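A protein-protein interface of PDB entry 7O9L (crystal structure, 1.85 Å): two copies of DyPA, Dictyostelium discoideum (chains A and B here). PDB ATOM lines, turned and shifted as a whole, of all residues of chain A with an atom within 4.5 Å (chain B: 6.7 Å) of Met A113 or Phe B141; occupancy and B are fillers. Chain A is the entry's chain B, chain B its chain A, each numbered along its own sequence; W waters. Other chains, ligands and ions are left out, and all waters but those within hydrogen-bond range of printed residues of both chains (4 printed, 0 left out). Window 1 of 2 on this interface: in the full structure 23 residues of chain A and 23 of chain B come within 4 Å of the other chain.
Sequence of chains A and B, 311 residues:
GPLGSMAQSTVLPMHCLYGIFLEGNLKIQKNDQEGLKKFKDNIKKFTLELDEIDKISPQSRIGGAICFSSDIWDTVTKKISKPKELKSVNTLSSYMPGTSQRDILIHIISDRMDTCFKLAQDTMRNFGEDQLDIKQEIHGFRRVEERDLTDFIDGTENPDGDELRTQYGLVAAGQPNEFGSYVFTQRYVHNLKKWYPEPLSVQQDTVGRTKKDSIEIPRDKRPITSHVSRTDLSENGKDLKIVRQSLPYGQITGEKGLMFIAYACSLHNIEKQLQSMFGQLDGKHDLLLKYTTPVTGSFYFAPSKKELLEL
The side-chain hydroxyl of Tyr B18 is in hydrogen-bond range of the side-chain hydroxyl of Tyr A18. The backbone NH (N) of Met A113 is in hydrogen-bond range of the side-chain hydroxyl (OH) of Tyr B18. The backbone NH (N) of Met B113 lies within hydrogen-bond range of the side-chain hydroxyl (OH) of Tyr A18 (3.1 Å).
O of Cys B16 is in hydrogen-bond range of NE of Arg B142 (2.9 Å). The backbone NH (N) of Arg B142 sits at hydrogen-bond distance from the backbone carbonyl oxygen (O) of Leu B17 (2.8 Å). N of Phe B141 lies within hydrogen-bond range of O of Pro B248 (3.0 Å). The guanidinium group (NH1) of Arg B143 sits at hydrogen-bond distance from the backbone carbonyl oxygen (O) of Arg B147 (3.0 Å). The side-chain carboxylate (OD2) of Asp A114 lies within salt-bridge range of the guanidinium group (NH2) of Arg A112, at 2.9 Å. The side-chain hydroxyl (OG1) of Thr A115 lies within hydrogen-bond range of the backbone carbonyl oxygen (O) of Arg A112 (3.4 Å).
Among the printed residues, merely in contact across the chains: His A139 with Gly B250 (3.1 Å), Asp A114 with Arg B142 (3.4 Å), Phe A117 with Phe B141 (3.5 Å), Phe A117 with Arg B143 (3.6 Å), Asp A114 with Val B144 (3.7 Å), His A139 with Gln B251 (3.7 Å), Asp A114 with Arg B143 (3.8 Å), Arg A112 with Leu B17 (3.9 Å) and Met A113 with Phe B141 (3.97 Å).
Of the printed residues of chain B, Met A113 touches Tyr B18 (3.1 Å) and Phe B141 (3.97 Å). Phe B141 touches just these residues of chain A: Met A113 (3.97 Å) and Phe A117 (3.5 Å). Printed residues of chain B within 4 Å of Arg A112: Leu B17. Printed residues of chain A within 4 Å of Arg B143: Asp A114 and Phe A117. Arg B147 touches none of the printed residues of chain A. Asp A111 touches none of the printed residues of chain B. The nearest residue of chain B that does not touch Met A113 is Arg B142 (5.0 Å). The nearest printed residue of chain A that does not touch Phe B141 is His A139 (4.9 Å). The nearest printed residue of chain B that does not touch His A139 is Phe B141 (4.9 Å).
Of the 10 printed residues of chain A, 6 touch a printed residue of chain B. Printed residues of chain A that touch a printed residue of chain B: Tyr A18, Arg A112, Met A113, Asp A114, Phe A117 and His A139. Hydrophobic or aromatic side chains of chain A within 4 Å of the printed part of chain B: Tyr A18, Met A113, Phe A117 and His A139. Along chain A the printed residues that touch a printed residue of chain B span positions 18 to 139.
Tyr A18 touches its own counterpart, Tyr B18. Tyr A18 touches Met B113, and with the chains exchanged Met A113 touches Tyr B18. Positions printed for both chains: 18, 113 and 139. Of the 12 pairs that touch across the chains among the printed residues, 3 have their exchanged pair printed and touching as well.
Water W4 bridges O of Asp A114 and N of Val B144. Water W3 lies within hydrogen-bond range of OD2 of Asp A114 (2.7 Å) and O of Arg B143 (2.9 Å). Water W2 lies within hydrogen-bond range of N of Asp A114 (3.1 Å) and OH of Tyr B18 (3.4 Å). Water W1 bridges OH of Tyr A18 and N of Met B113.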
ATOM      1  N   TYR A  18      22.390  26.747   3.823  1.00  0.00           N
ATOM      2  CA  TYR A  18      22.880  25.448   3.378  1.00  0.00           C
ATOM      3  C   TYR A  18      23.170  24.593   4.601  1.00  0.00           C
ATOM      4  O   TYR A  18      23.528  25.105   5.663  1.00  0.00           O
ATOM      5  CB  TYR A  18      24.154  25.567   2.511  1.00  0.00           C
ATOM      6  CG  TYR A  18      23.942  26.485   1.343  1.00  0.00           C
ATOM      7  CD1 TYR A  18      23.418  25.999   0.145  1.00  0.00           C
ATOM      8  CD2 TYR A  18      24.185  27.850   1.457  1.00  0.00           C
ATOM      9  CE1 TYR A  18      23.174  26.844  -0.917  1.00  0.00           C
ATOM     10  CE2 TYR A  18      23.931  28.710   0.398  1.00  0.00           C
ATOM     11  CZ  TYR A  18      23.422  28.193  -0.788  1.00  0.00           C
ATOM     12  OH  TYR A  18      23.161  29.043  -1.839  1.00  0.00           O
ATOM     13  N   ILE A  20      24.949  20.471   5.455  1.00  0.00           N
ATOM     14  CA  ILE A  20      25.407  19.167   4.999  1.00  0.00           C
ATOM     15  C   ILE A  20      25.259  18.211   6.171  1.00  0.00           C
ATOM     16  O   ILE A  20      25.610  18.553   7.307  1.00  0.00           O
ATOM     17  CB  ILE A  20      26.850  19.218   4.462  1.00  0.00           C
ATOM     18  CG1 ILE A  20      26.855  19.969   3.119  1.00  0.00           C
ATOM     19  CG2 ILE A  20      27.389  17.802   4.253  1.00  0.00           C
ATOM     20  CD1 ILE A  20      28.246  20.130   2.476  1.00  0.00           C
ATOM     21  N   ASP A 111      25.856  29.955   5.298  1.00  0.00           N
ATOM     22  CA  ASP A 111      25.170  30.764   4.301  1.00  0.00           C
ATOM     23  C   ASP A 111      25.834  30.692   2.930  1.00  0.00           C
ATOM     24  O   ASP A 111      25.359  31.351   1.994  1.00  0.00           O
ATOM     25  CB  ASP A 111      25.097  32.225   4.742  1.00  0.00           C
ATOM     26  CG  ASP A 111      24.084  32.450   5.846  1.00  0.00           C
ATOM     27  OD1 ASP A 111      23.479  31.462   6.316  1.00  0.00           O
ATOM     28  OD2 ASP A 111      23.890  33.624   6.222  1.00  0.00           O
ATOM     29  N   ARG A 112      26.887  29.884   2.773  1.00  0.00           N
ATOM     30  CA  ARG A 112      27.522  29.668   1.475  1.00  0.00           C
ATOM     31  C   ARG A 112      27.786  28.183   1.297  1.00  0.00           C
ATOM     32  O   ARG A 112      28.337  27.544   2.197  1.00  0.00           O
ATOM     33  CB  ARG A 112      28.867  30.423   1.358  1.00  0.00           C
ATOM     34  CG  ARG A 112      28.784  31.932   1.518  1.00  0.00           C
ATOM     35  CD  ARG A 112      30.163  32.585   1.387  1.00  0.00           C
ATOM     36  NE  ARG A 112      30.803  32.251   0.114  1.00  0.00           N
ATOM     37  CZ  ARG A 112      30.756  33.027  -0.964  1.00  0.00           C
ATOM     38  NH1 ARG A 112      30.110  34.192  -0.915  1.00  0.00           N
ATOM     39  NH2 ARG A 112      31.372  32.653  -2.083  1.00  0.00           N
ATOM     40  N   MET A 113      27.445  27.644   0.130  1.00  0.00           N
ATOM     41  CA  MET A 113      27.786  26.246  -0.114  1.00  0.00           C
ATOM     42  C   MET A 113      29.296  26.023  -0.177  1.00  0.00           C
ATOM     43  O   MET A 113      29.763  24.952   0.217  1.00  0.00           O
ATOM     44  CB  MET A 113      27.128  25.747  -1.401  1.00  0.00           C
ATOM     45  CG  MET A 113      27.354  24.252  -1.686  1.00  0.00           C
ATOM     46  SD  MET A 113      26.725  23.130  -0.397  1.00  0.00           S
ATOM     47  CE  MET A 113      26.940  21.526  -1.204  1.00  0.00           C
ATOM     48  N   ASP A 114      30.085  26.989  -0.668  1.00  0.00           N
ATOM     49  CA  ASP A 114      31.501  26.661  -0.846  1.00  0.00           C
ATOM     50  C   ASP A 114      32.181  26.393   0.496  1.00  0.00           C
ATOM     51  O   ASP A 114      32.961  25.438   0.614  1.00  0.00           O
ATOM     52  CB  ASP A 114      32.246  27.727  -1.678  1.00  0.00           C
ATOM     53  CG  ASP A 114      32.170  29.151  -1.120  1.00  0.00           C
ATOM     54  OD1 ASP A 114      31.679  29.389   0.006  1.00  0.00           O
ATOM     55  OD2 ASP A 114      32.642  30.056  -1.854  1.00  0.00           O
ATOM     56  N   THR A 115      31.847  27.166   1.542  1.00  0.00           N
ATOM     57  CA  THR A 115      32.478  26.904   2.838  1.00  0.00           C
ATOM     58  C   THR A 115      31.842  25.724   3.558  1.00  0.00           C
ATOM     59  O   THR A 115      32.547  24.978   4.250  1.00  0.00           O
ATOM     60  CB  THR A 115      32.445  28.155   3.731  1.00  0.00           C
ATOM     61  OG1 THR A 115      31.118  28.686   3.788  1.00  0.00           O
ATOM     62  CG2 THR A 115      33.371  29.222   3.169  1.00  0.00           C
ATOM     63  N   CYS A 116      30.528  25.540   3.401  1.00  0.00           N
ATOM     64  CA  CYS A 116      29.867  24.334   3.886  1.00  0.00           C
ATOM     65  C   CYS A 116      30.569  23.090   3.339  1.00  0.00           C
ATOM     66  O   CYS A 116      30.996  22.203   4.091  1.00  0.00           O
ATOM     67  CB  CYS A 116      28.401  24.371   3.436  1.00  0.00           C
ATOM     68  SG  CYS A 116      27.290  23.368   4.429  1.00  0.00           S
ATOM     69  N   PHE A 117      30.711  23.028   2.014  1.00  0.00           N
ATOM     70  CA  PHE A 117      31.357  21.882   1.372  1.00  0.00           C
ATOM     71  C   PHE A 117      32.826  21.756   1.769  1.00  0.00           C
ATOM     72  O   PHE A 117      33.322  20.642   1.973  1.00  0.00           O
ATOM     73  CB  PHE A 117      31.216  22.017  -0.141  1.00  0.00           C
ATOM     74  CG  PHE A 117      31.663  20.808  -0.916  1.00  0.00           C
ATOM     75  CD1 PHE A 117      30.780  19.780  -1.188  1.00  0.00           C
ATOM     76  CD2 PHE A 117      32.973  20.706  -1.358  1.00  0.00           C
ATOM     77  CE1 PHE A 117      31.183  18.671  -1.913  1.00  0.00           C
ATOM     78  CE2 PHE A 117      33.380  19.595  -2.077  1.00  0.00           C
ATOM     79  CZ  PHE A 117      32.480  18.581  -2.350  1.00  0.00           C
ATOM     80  N   HIS A 139      22.777  17.040   1.039  1.00  0.00           N
ATOM     81  CA  HIS A 139      23.059  18.458   0.827  1.00  0.00           C
ATOM     82  C   HIS A 139      21.731  19.192   0.915  1.00  0.00           C
ATOM     83  O   HIS A 139      20.929  19.151  -0.019  1.00  0.00           O
ATOM     84  CB  HIS A 139      23.722  18.700  -0.527  1.00  0.00           C
ATOM     85  CG  HIS A 139      25.055  18.037  -0.672  1.00  0.00           C
ATOM     86  ND1 HIS A 139      25.754  18.034  -1.864  1.00  0.00           N
ATOM     87  CD2 HIS A 139      25.813  17.347   0.213  1.00  0.00           C
ATOM     88  CE1 HIS A 139      26.893  17.377  -1.702  1.00  0.00           C
ATOM     89  NE2 HIS A 139      26.951  16.944  -0.454  1.00  0.00           N
ATOM     90  N   CYS B  16      29.664  32.619 -11.721  1.00  0.00           N
ATOM     91  CA  CYS B  16      28.465  32.162 -11.015  1.00  0.00           C
ATOM     92  C   CYS B  16      28.831  31.186  -9.902  1.00  0.00           C
ATOM     93  O   CYS B  16      29.823  30.458  -9.990  1.00  0.00           O
ATOM     94  CB  CYS B  16      27.488  31.492 -11.985  1.00  0.00           C
ATOM     95  SG  CYS B  16      28.194  30.012 -12.846  1.00  0.00           S
ATOM     96  N   LEU B  17      28.041  31.201  -8.819  1.00  0.00           N
ATOM     97  CA  LEU B  17      28.321  30.316  -7.692  1.00  0.00           C
ATOM     98  C   LEU B  17      27.533  29.015  -7.753  1.00  0.00           C
ATOM     99  O   LEU B  17      27.929  28.039  -7.103  1.00  0.00           O
ATOM    100  CB  LEU B  17      28.010  31.033  -6.366  1.00  0.00           C
ATOM    101  CG  LEU B  17      28.834  32.292  -6.082  1.00  0.00           C
ATOM    102  CD1 LEU B  17      28.484  32.907  -4.724  1.00  0.00           C
ATOM    103  CD2 LEU B  17      30.331  31.939  -6.148  1.00  0.00           C
ATOM    104  N   TYR B  18      26.434  28.987  -8.514  1.00  0.00           N
ATOM    105  CA  TYR B  18      25.561  27.827  -8.627  1.00  0.00           C
ATOM    106  C   TYR B  18      25.123  27.667 -10.072  1.00  0.00           C
ATOM    107  O   TYR B  18      24.972  28.644 -10.806  1.00  0.00           O
ATOM    108  CB  TYR B  18      24.311  27.932  -7.728  1.00  0.00           C
ATOM    109  CG  TYR B  18      24.701  28.155  -6.287  1.00  0.00           C
ATOM    110  CD1 TYR B  18      25.022  27.081  -5.465  1.00  0.00           C
ATOM    111  CD2 TYR B  18      24.844  29.435  -5.786  1.00  0.00           C
ATOM    112  CE1 TYR B  18      25.431  27.276  -4.165  1.00  0.00           C
ATOM    113  CE2 TYR B  18      25.265  29.649  -4.472  1.00  0.00           C
ATOM    114  CZ  TYR B  18      25.547  28.556  -3.669  1.00  0.00           C
ATOM    115  OH  TYR B  18      25.976  28.743  -2.371  1.00  0.00           O
ATOM    116  N   GLY B  19      24.909  26.422 -10.461  1.00  0.00           N
ATOM    117  CA  GLY B  19      24.316  26.176 -11.759  1.00  0.00           C
ATOM    118  C   GLY B  19      23.466  24.928 -11.706  1.00  0.00           C
ATOM    119  O   GLY B  19      23.842  23.947 -11.065  1.00  0.00           O
ATOM    120  N   PHE B  21      21.661  22.088 -14.225  1.00  0.00           N
ATOM    121  CA  PHE B  21      21.707  21.567 -15.588  1.00  0.00           C
ATOM    122  C   PHE B  21      20.611  20.524 -15.740  1.00  0.00           C
ATOM    123  O   PHE B  21      20.612  19.513 -15.029  1.00  0.00           O
ATOM    124  CB  PHE B  21      23.065  20.930 -15.900  1.00  0.00           C
ATOM    125  CG  PHE B  21      24.255  21.839 -15.665  1.00  0.00           C
ATOM    126  CD1 PHE B  21      24.696  22.119 -14.377  1.00  0.00           C
ATOM    127  CD2 PHE B  21      24.952  22.376 -16.745  1.00  0.00           C
ATOM    128  CE1 PHE B  21      25.793  22.947 -14.170  1.00  0.00           C
ATOM    129  CE2 PHE B  21      26.057  23.200 -16.547  1.00  0.00           C
ATOM    130  CZ  PHE B  21      26.480  23.474 -15.259  1.00  0.00           C
ATOM    131  N   MET B 113      21.600  29.632  -4.449  1.00  0.00           N
ATOM    132  CA  MET B 113      20.892  28.414  -4.828  1.00  0.00           C
ATOM    133  C   MET B 113      19.377  28.599  -4.765  1.00  0.00           C
ATOM    134  O   MET B 113      18.653  27.987  -5.562  1.00  0.00           O
ATOM    135  CB  MET B 113      21.317  27.240  -3.943  1.00  0.00           C
ATOM    136  CG  MET B 113      20.608  25.915  -4.249  1.00  0.00           C
ATOM    137  SD  MET B 113      20.959  25.285  -5.920  1.00  0.00           S
ATOM    138  CE  MET B 113      20.224  23.638  -5.833  1.00  0.00           C
ATOM    139  N   HIS B 139      23.157  19.540  -9.964  1.00  0.00           N
ATOM    140  CA  HIS B 139      23.276  20.757  -9.175  1.00  0.00           C
ATOM    141  C   HIS B 139      24.768  21.059  -9.028  1.00  0.00           C
ATOM    142  O   HIS B 139      25.460  20.421  -8.236  1.00  0.00           O
ATOM    143  CB  HIS B 139      22.620  20.589  -7.809  1.00  0.00           C
ATOM    144  CG  HIS B 139      21.153  20.291  -7.872  1.00  0.00           C
ATOM    145  ND1 HIS B 139      20.396  20.045  -6.743  1.00  0.00           N
ATOM    146  CD2 HIS B 139      20.304  20.196  -8.925  1.00  0.00           C
ATOM    147  CE1 HIS B 139      19.143  19.811  -7.103  1.00  0.00           C
ATOM    148  NE2 HIS B 139      19.061  19.902  -8.420  1.00  0.00           N
ATOM    149  N   GLY B 140      25.267  22.022  -9.799  1.00  0.00           N
ATOM    150  CA  GLY B 140      26.667  22.423  -9.697  1.00  0.00           C
ATOM    151  C   GLY B 140      26.849  23.555  -8.696  1.00  0.00           C
ATOM    152  O   GLY B 140      25.947  24.370  -8.475  1.00  0.00           O
ATOM    153  N   PHE B 141      28.034  23.600  -8.086  1.00  0.00           N
ATOM    154  CA  PHE B 141      28.357  24.661  -7.141  1.00  0.00           C
ATOM    155  C   PHE B 141      29.839  24.990  -7.229  1.00  0.00           C
ATOM    156  O   PHE B 141      30.685  24.098  -7.353  1.00  0.00           O
ATOM    157  CB  PHE B 141      27.994  24.285  -5.690  1.00  0.00           C
ATOM    158  CG  PHE B 141      28.561  22.970  -5.247  1.00  0.00           C
ATOM    159  CD1 PHE B 141      27.875  21.787  -5.489  1.00  0.00           C
ATOM    160  CD2 PHE B 141      29.785  22.915  -4.592  1.00  0.00           C
ATOM    161  CE1 PHE B 141      28.400  20.572  -5.082  1.00  0.00           C
ATOM    162  CE2 PHE B 141      30.319  21.704  -4.192  1.00  0.00           C
ATOM    163  CZ  PHE B 141      29.626  20.529  -4.444  1.00  0.00           C
ATOM    164  N   ARG B 142      30.140  26.281  -7.132  1.00  0.00           N
ATOM    165  CA  ARG B 142      31.522  26.728  -7.088  1.00  0.00           C
ATOM    166  C   ARG B 142      32.130  26.380  -5.736  1.00  0.00           C
ATOM    167  O   ARG B 142      31.469  26.483  -4.695  1.00  0.00           O
ATOM    168  CB  ARG B 142      31.575  28.234  -7.328  1.00  0.00           C
ATOM    169  CG  ARG B 142      32.959  28.794  -7.585  1.00  0.00           C
ATOM    170  CD  ARG B 142      33.353  28.571  -9.062  1.00  0.00           C
ATOM    171  NE  ARG B 142      32.472  29.271  -9.999  1.00  0.00           N
ATOM    172  CZ  ARG B 142      32.653  29.284 -11.320  1.00  0.00           C
ATOM    173  NH1 ARG B 142      33.687  28.642 -11.858  1.00  0.00           N
ATOM    174  NH2 ARG B 142      31.815  29.950 -12.104  1.00  0.00           N
ATOM    175  N   ARG B 143      33.393  25.959  -5.752  1.00  0.00           N
ATOM    176  CA  ARG B 143      34.129  25.672  -4.529  1.00  0.00           C
ATOM    177  C   ARG B 143      35.017  26.855  -4.159  1.00  0.00           C
ATOM    178  O   ARG B 143      35.212  27.786  -4.943  1.00  0.00           O
ATOM    179  CB  ARG B 143      34.975  24.402  -4.705  1.00  0.00           C
ATOM    180  CG  ARG B 143      34.110  23.144  -4.635  1.00  0.00           C
ATOM    181  CD  ARG B 143      34.918  21.895  -4.964  1.00  0.00           C
ATOM    182  NE  ARG B 143      35.844  21.476  -3.899  1.00  0.00           N
ATOM    183  CZ  ARG B 143      37.166  21.376  -4.070  1.00  0.00           C
ATOM    184  NH1 ARG B 143      37.706  21.739  -5.219  1.00  0.00           N
ATOM    185  NH2 ARG B 143      37.954  20.941  -3.092  1.00  0.00           N
ATOM    186  N   VAL B 144      35.574  26.802  -2.943  1.00  0.00           N
ATOM    187  CA  VAL B 144      36.477  27.856  -2.496  1.00  0.00           C
ATOM    188  C   VAL B 144      37.626  28.030  -3.494  1.00  0.00           C
ATOM    189  O   VAL B 144      38.193  27.054  -4.003  1.00  0.00           O
ATOM    190  CB  VAL B 144      36.988  27.541  -1.075  1.00  0.00           C
ATOM    191  CG1 VAL B 144      38.127  28.477  -0.693  1.00  0.00           C
ATOM    192  CG2 VAL B 144      35.838  27.651  -0.054  1.00  0.00           C
ATOM    193  N   ARG B 147      38.229  26.335  -7.325  1.00  0.00           N
ATOM    194  CA  ARG B 147      39.006  25.155  -7.671  1.00  0.00           C
ATOM    195  C   ARG B 147      38.114  23.990  -8.087  1.00  0.00           C
ATOM    196  O   ARG B 147      37.094  23.709  -7.448  1.00  0.00           O
ATOM    197  CB  ARG B 147      39.897  24.761  -6.493  1.00  0.00           C
ATOM    198  CG  ARG B 147      40.999  25.790  -6.268  1.00  0.00           C
ATOM    199  CD  ARG B 147      41.899  25.436  -5.085  1.00  0.00           C
ATOM    200  NE  ARG B 147      42.813  26.545  -4.812  1.00  0.00           N
ATOM    201  CZ  ARG B 147      44.004  26.683  -5.391  1.00  0.00           C
ATOM    202  NH1 ARG B 147      44.438  25.783  -6.277  1.00  0.00           N
ATOM    203  NH2 ARG B 147      44.764  27.731  -5.088  1.00  0.00           N
ATOM    204  N   LEU B 149      37.635  19.898  -8.372  1.00  0.00           N
ATOM    205  CA  LEU B 149      37.935  18.904  -7.337  1.00  0.00           C
ATOM    206  C   LEU B 149      39.339  18.294  -7.461  1.00  0.00           C
ATOM    207  O   LEU B 149      39.812  17.677  -6.496  1.00  0.00           O
ATOM    208  CB  LEU B 149      36.863  17.806  -7.350  1.00  0.00           C
ATOM    209  CG  LEU B 149      35.556  18.222  -6.661  1.00  0.00           C
ATOM    210  CD1 LEU B 149      34.399  17.327  -7.093  1.00  0.00           C
ATOM    211  CD2 LEU B 149      35.733  18.227  -5.118  1.00  0.00           C
ATOM    212  N   LEU B 247      31.157  23.621 -13.595  1.00  0.00           N
ATOM    213  CA  LEU B 247      31.107  23.710 -12.120  1.00  0.00           C
ATOM    214  C   LEU B 247      31.294  22.327 -11.515  1.00  0.00           C
ATOM    215  O   LEU B 247      30.788  21.336 -12.069  1.00  0.00           O
ATOM    216  CB  LEU B 247      29.756  24.279 -11.625  1.00  0.00           C
ATOM    217  CG  LEU B 247      29.487  25.772 -11.779  1.00  0.00           C
ATOM    218  CD1 LEU B 247      28.050  26.067 -11.322  1.00  0.00           C
ATOM    219  CD2 LEU B 247      30.514  26.567 -10.968  1.00  0.00           C
ATOM    220  N   PRO B 248      31.971  22.232 -10.372  1.00  0.00           N
ATOM    221  CA  PRO B 248      31.982  20.973  -9.612  1.00  0.00           C
ATOM    222  C   PRO B 248      30.571  20.533  -9.238  1.00  0.00           C
ATOM    223  O   PRO B 248      29.644  21.339  -9.147  1.00  0.00           O
ATOM    224  CB  PRO B 248      32.790  21.325  -8.351  1.00  0.00           C
ATOM    225  CG  PRO B 248      33.612  22.542  -8.730  1.00  0.00           C
ATOM    226  CD  PRO B 248      32.814  23.284  -9.770  1.00  0.00           C
ATOM    227  N   TYR B 249      30.422  19.232  -8.971  1.00  0.00           N
ATOM    228  CA  TYR B 249      29.158  18.678  -8.471  1.00  0.00           C
ATOM    229  C   TYR B 249      29.484  17.407  -7.689  1.00  0.00           C
ATOM    230  O   TYR B 249      30.567  16.832  -7.840  1.00  0.00           O
ATOM    231  CB  TYR B 249      28.170  18.336  -9.616  1.00  0.00           C
ATOM    232  CG  TYR B 249      28.607  17.050 -10.292  1.00  0.00           C
ATOM    233  CD1 TYR B 249      29.600  17.064 -11.263  1.00  0.00           C
ATOM    234  CD2 TYR B 249      28.083  15.814  -9.903  1.00  0.00           C
ATOM    235  CE1 TYR B 249      30.050  15.884 -11.855  1.00  0.00           C
ATOM    236  CE2 TYR B 249      28.547  14.627 -10.468  1.00  0.00           C
ATOM    237  CZ  TYR B 249      29.523  14.679 -11.452  1.00  0.00           C
ATOM    238  OH  TYR B 249      29.994  13.513 -12.013  1.00  0.00           O
ATOM    239  N   GLY B 250      28.526  16.947  -6.877  1.00  0.00           N
ATOM    240  CA  GLY B 250      28.534  15.577  -6.396  1.00  0.00           C
ATOM    241  C   GLY B 250      28.643  15.461  -4.887  1.00  0.00           C
ATOM    242  O   GLY B 250      28.602  16.449  -4.144  1.00  0.00           O
ATOM    243  N   GLN B 251      28.808  14.213  -4.441  1.00  0.00           N
ATOM    244  CA  GLN B 251      28.878  13.846  -3.032  1.00  0.00           C
ATOM    245  C   GLN B 251      30.318  13.585  -2.615  1.00  0.00           C
ATOM    246  O   GLN B 251      31.054  12.883  -3.310  1.00  0.00           O
ATOM    247  CB  GLN B 251      28.065  12.579  -2.761  1.00  0.00           C
ATOM    248  CG  GLN B 251      26.635  12.618  -3.234  1.00  0.00           C
ATOM    249  CD  GLN B 251      25.676  12.811  -2.088  1.00  0.00           C
ATOM    250  OE1 GLN B 251      25.255  13.931  -1.808  1.00  0.00           O
ATOM    251  NE2 GLN B 251      25.329  11.718  -1.405  1.00  0.00           N
HETATM  252  O   HOH W   1      20.277  30.529  -1.431  1.00  0.00           O
HETATM  253  O   HOH W   2      29.244  29.526  -2.304  1.00  0.00           O
HETATM  254  O   HOH W   3      33.382  29.974  -4.489  1.00  0.00           O
HETATM  255  O   HOH W   4      34.455  24.502  -1.457  1.00  0.00           O
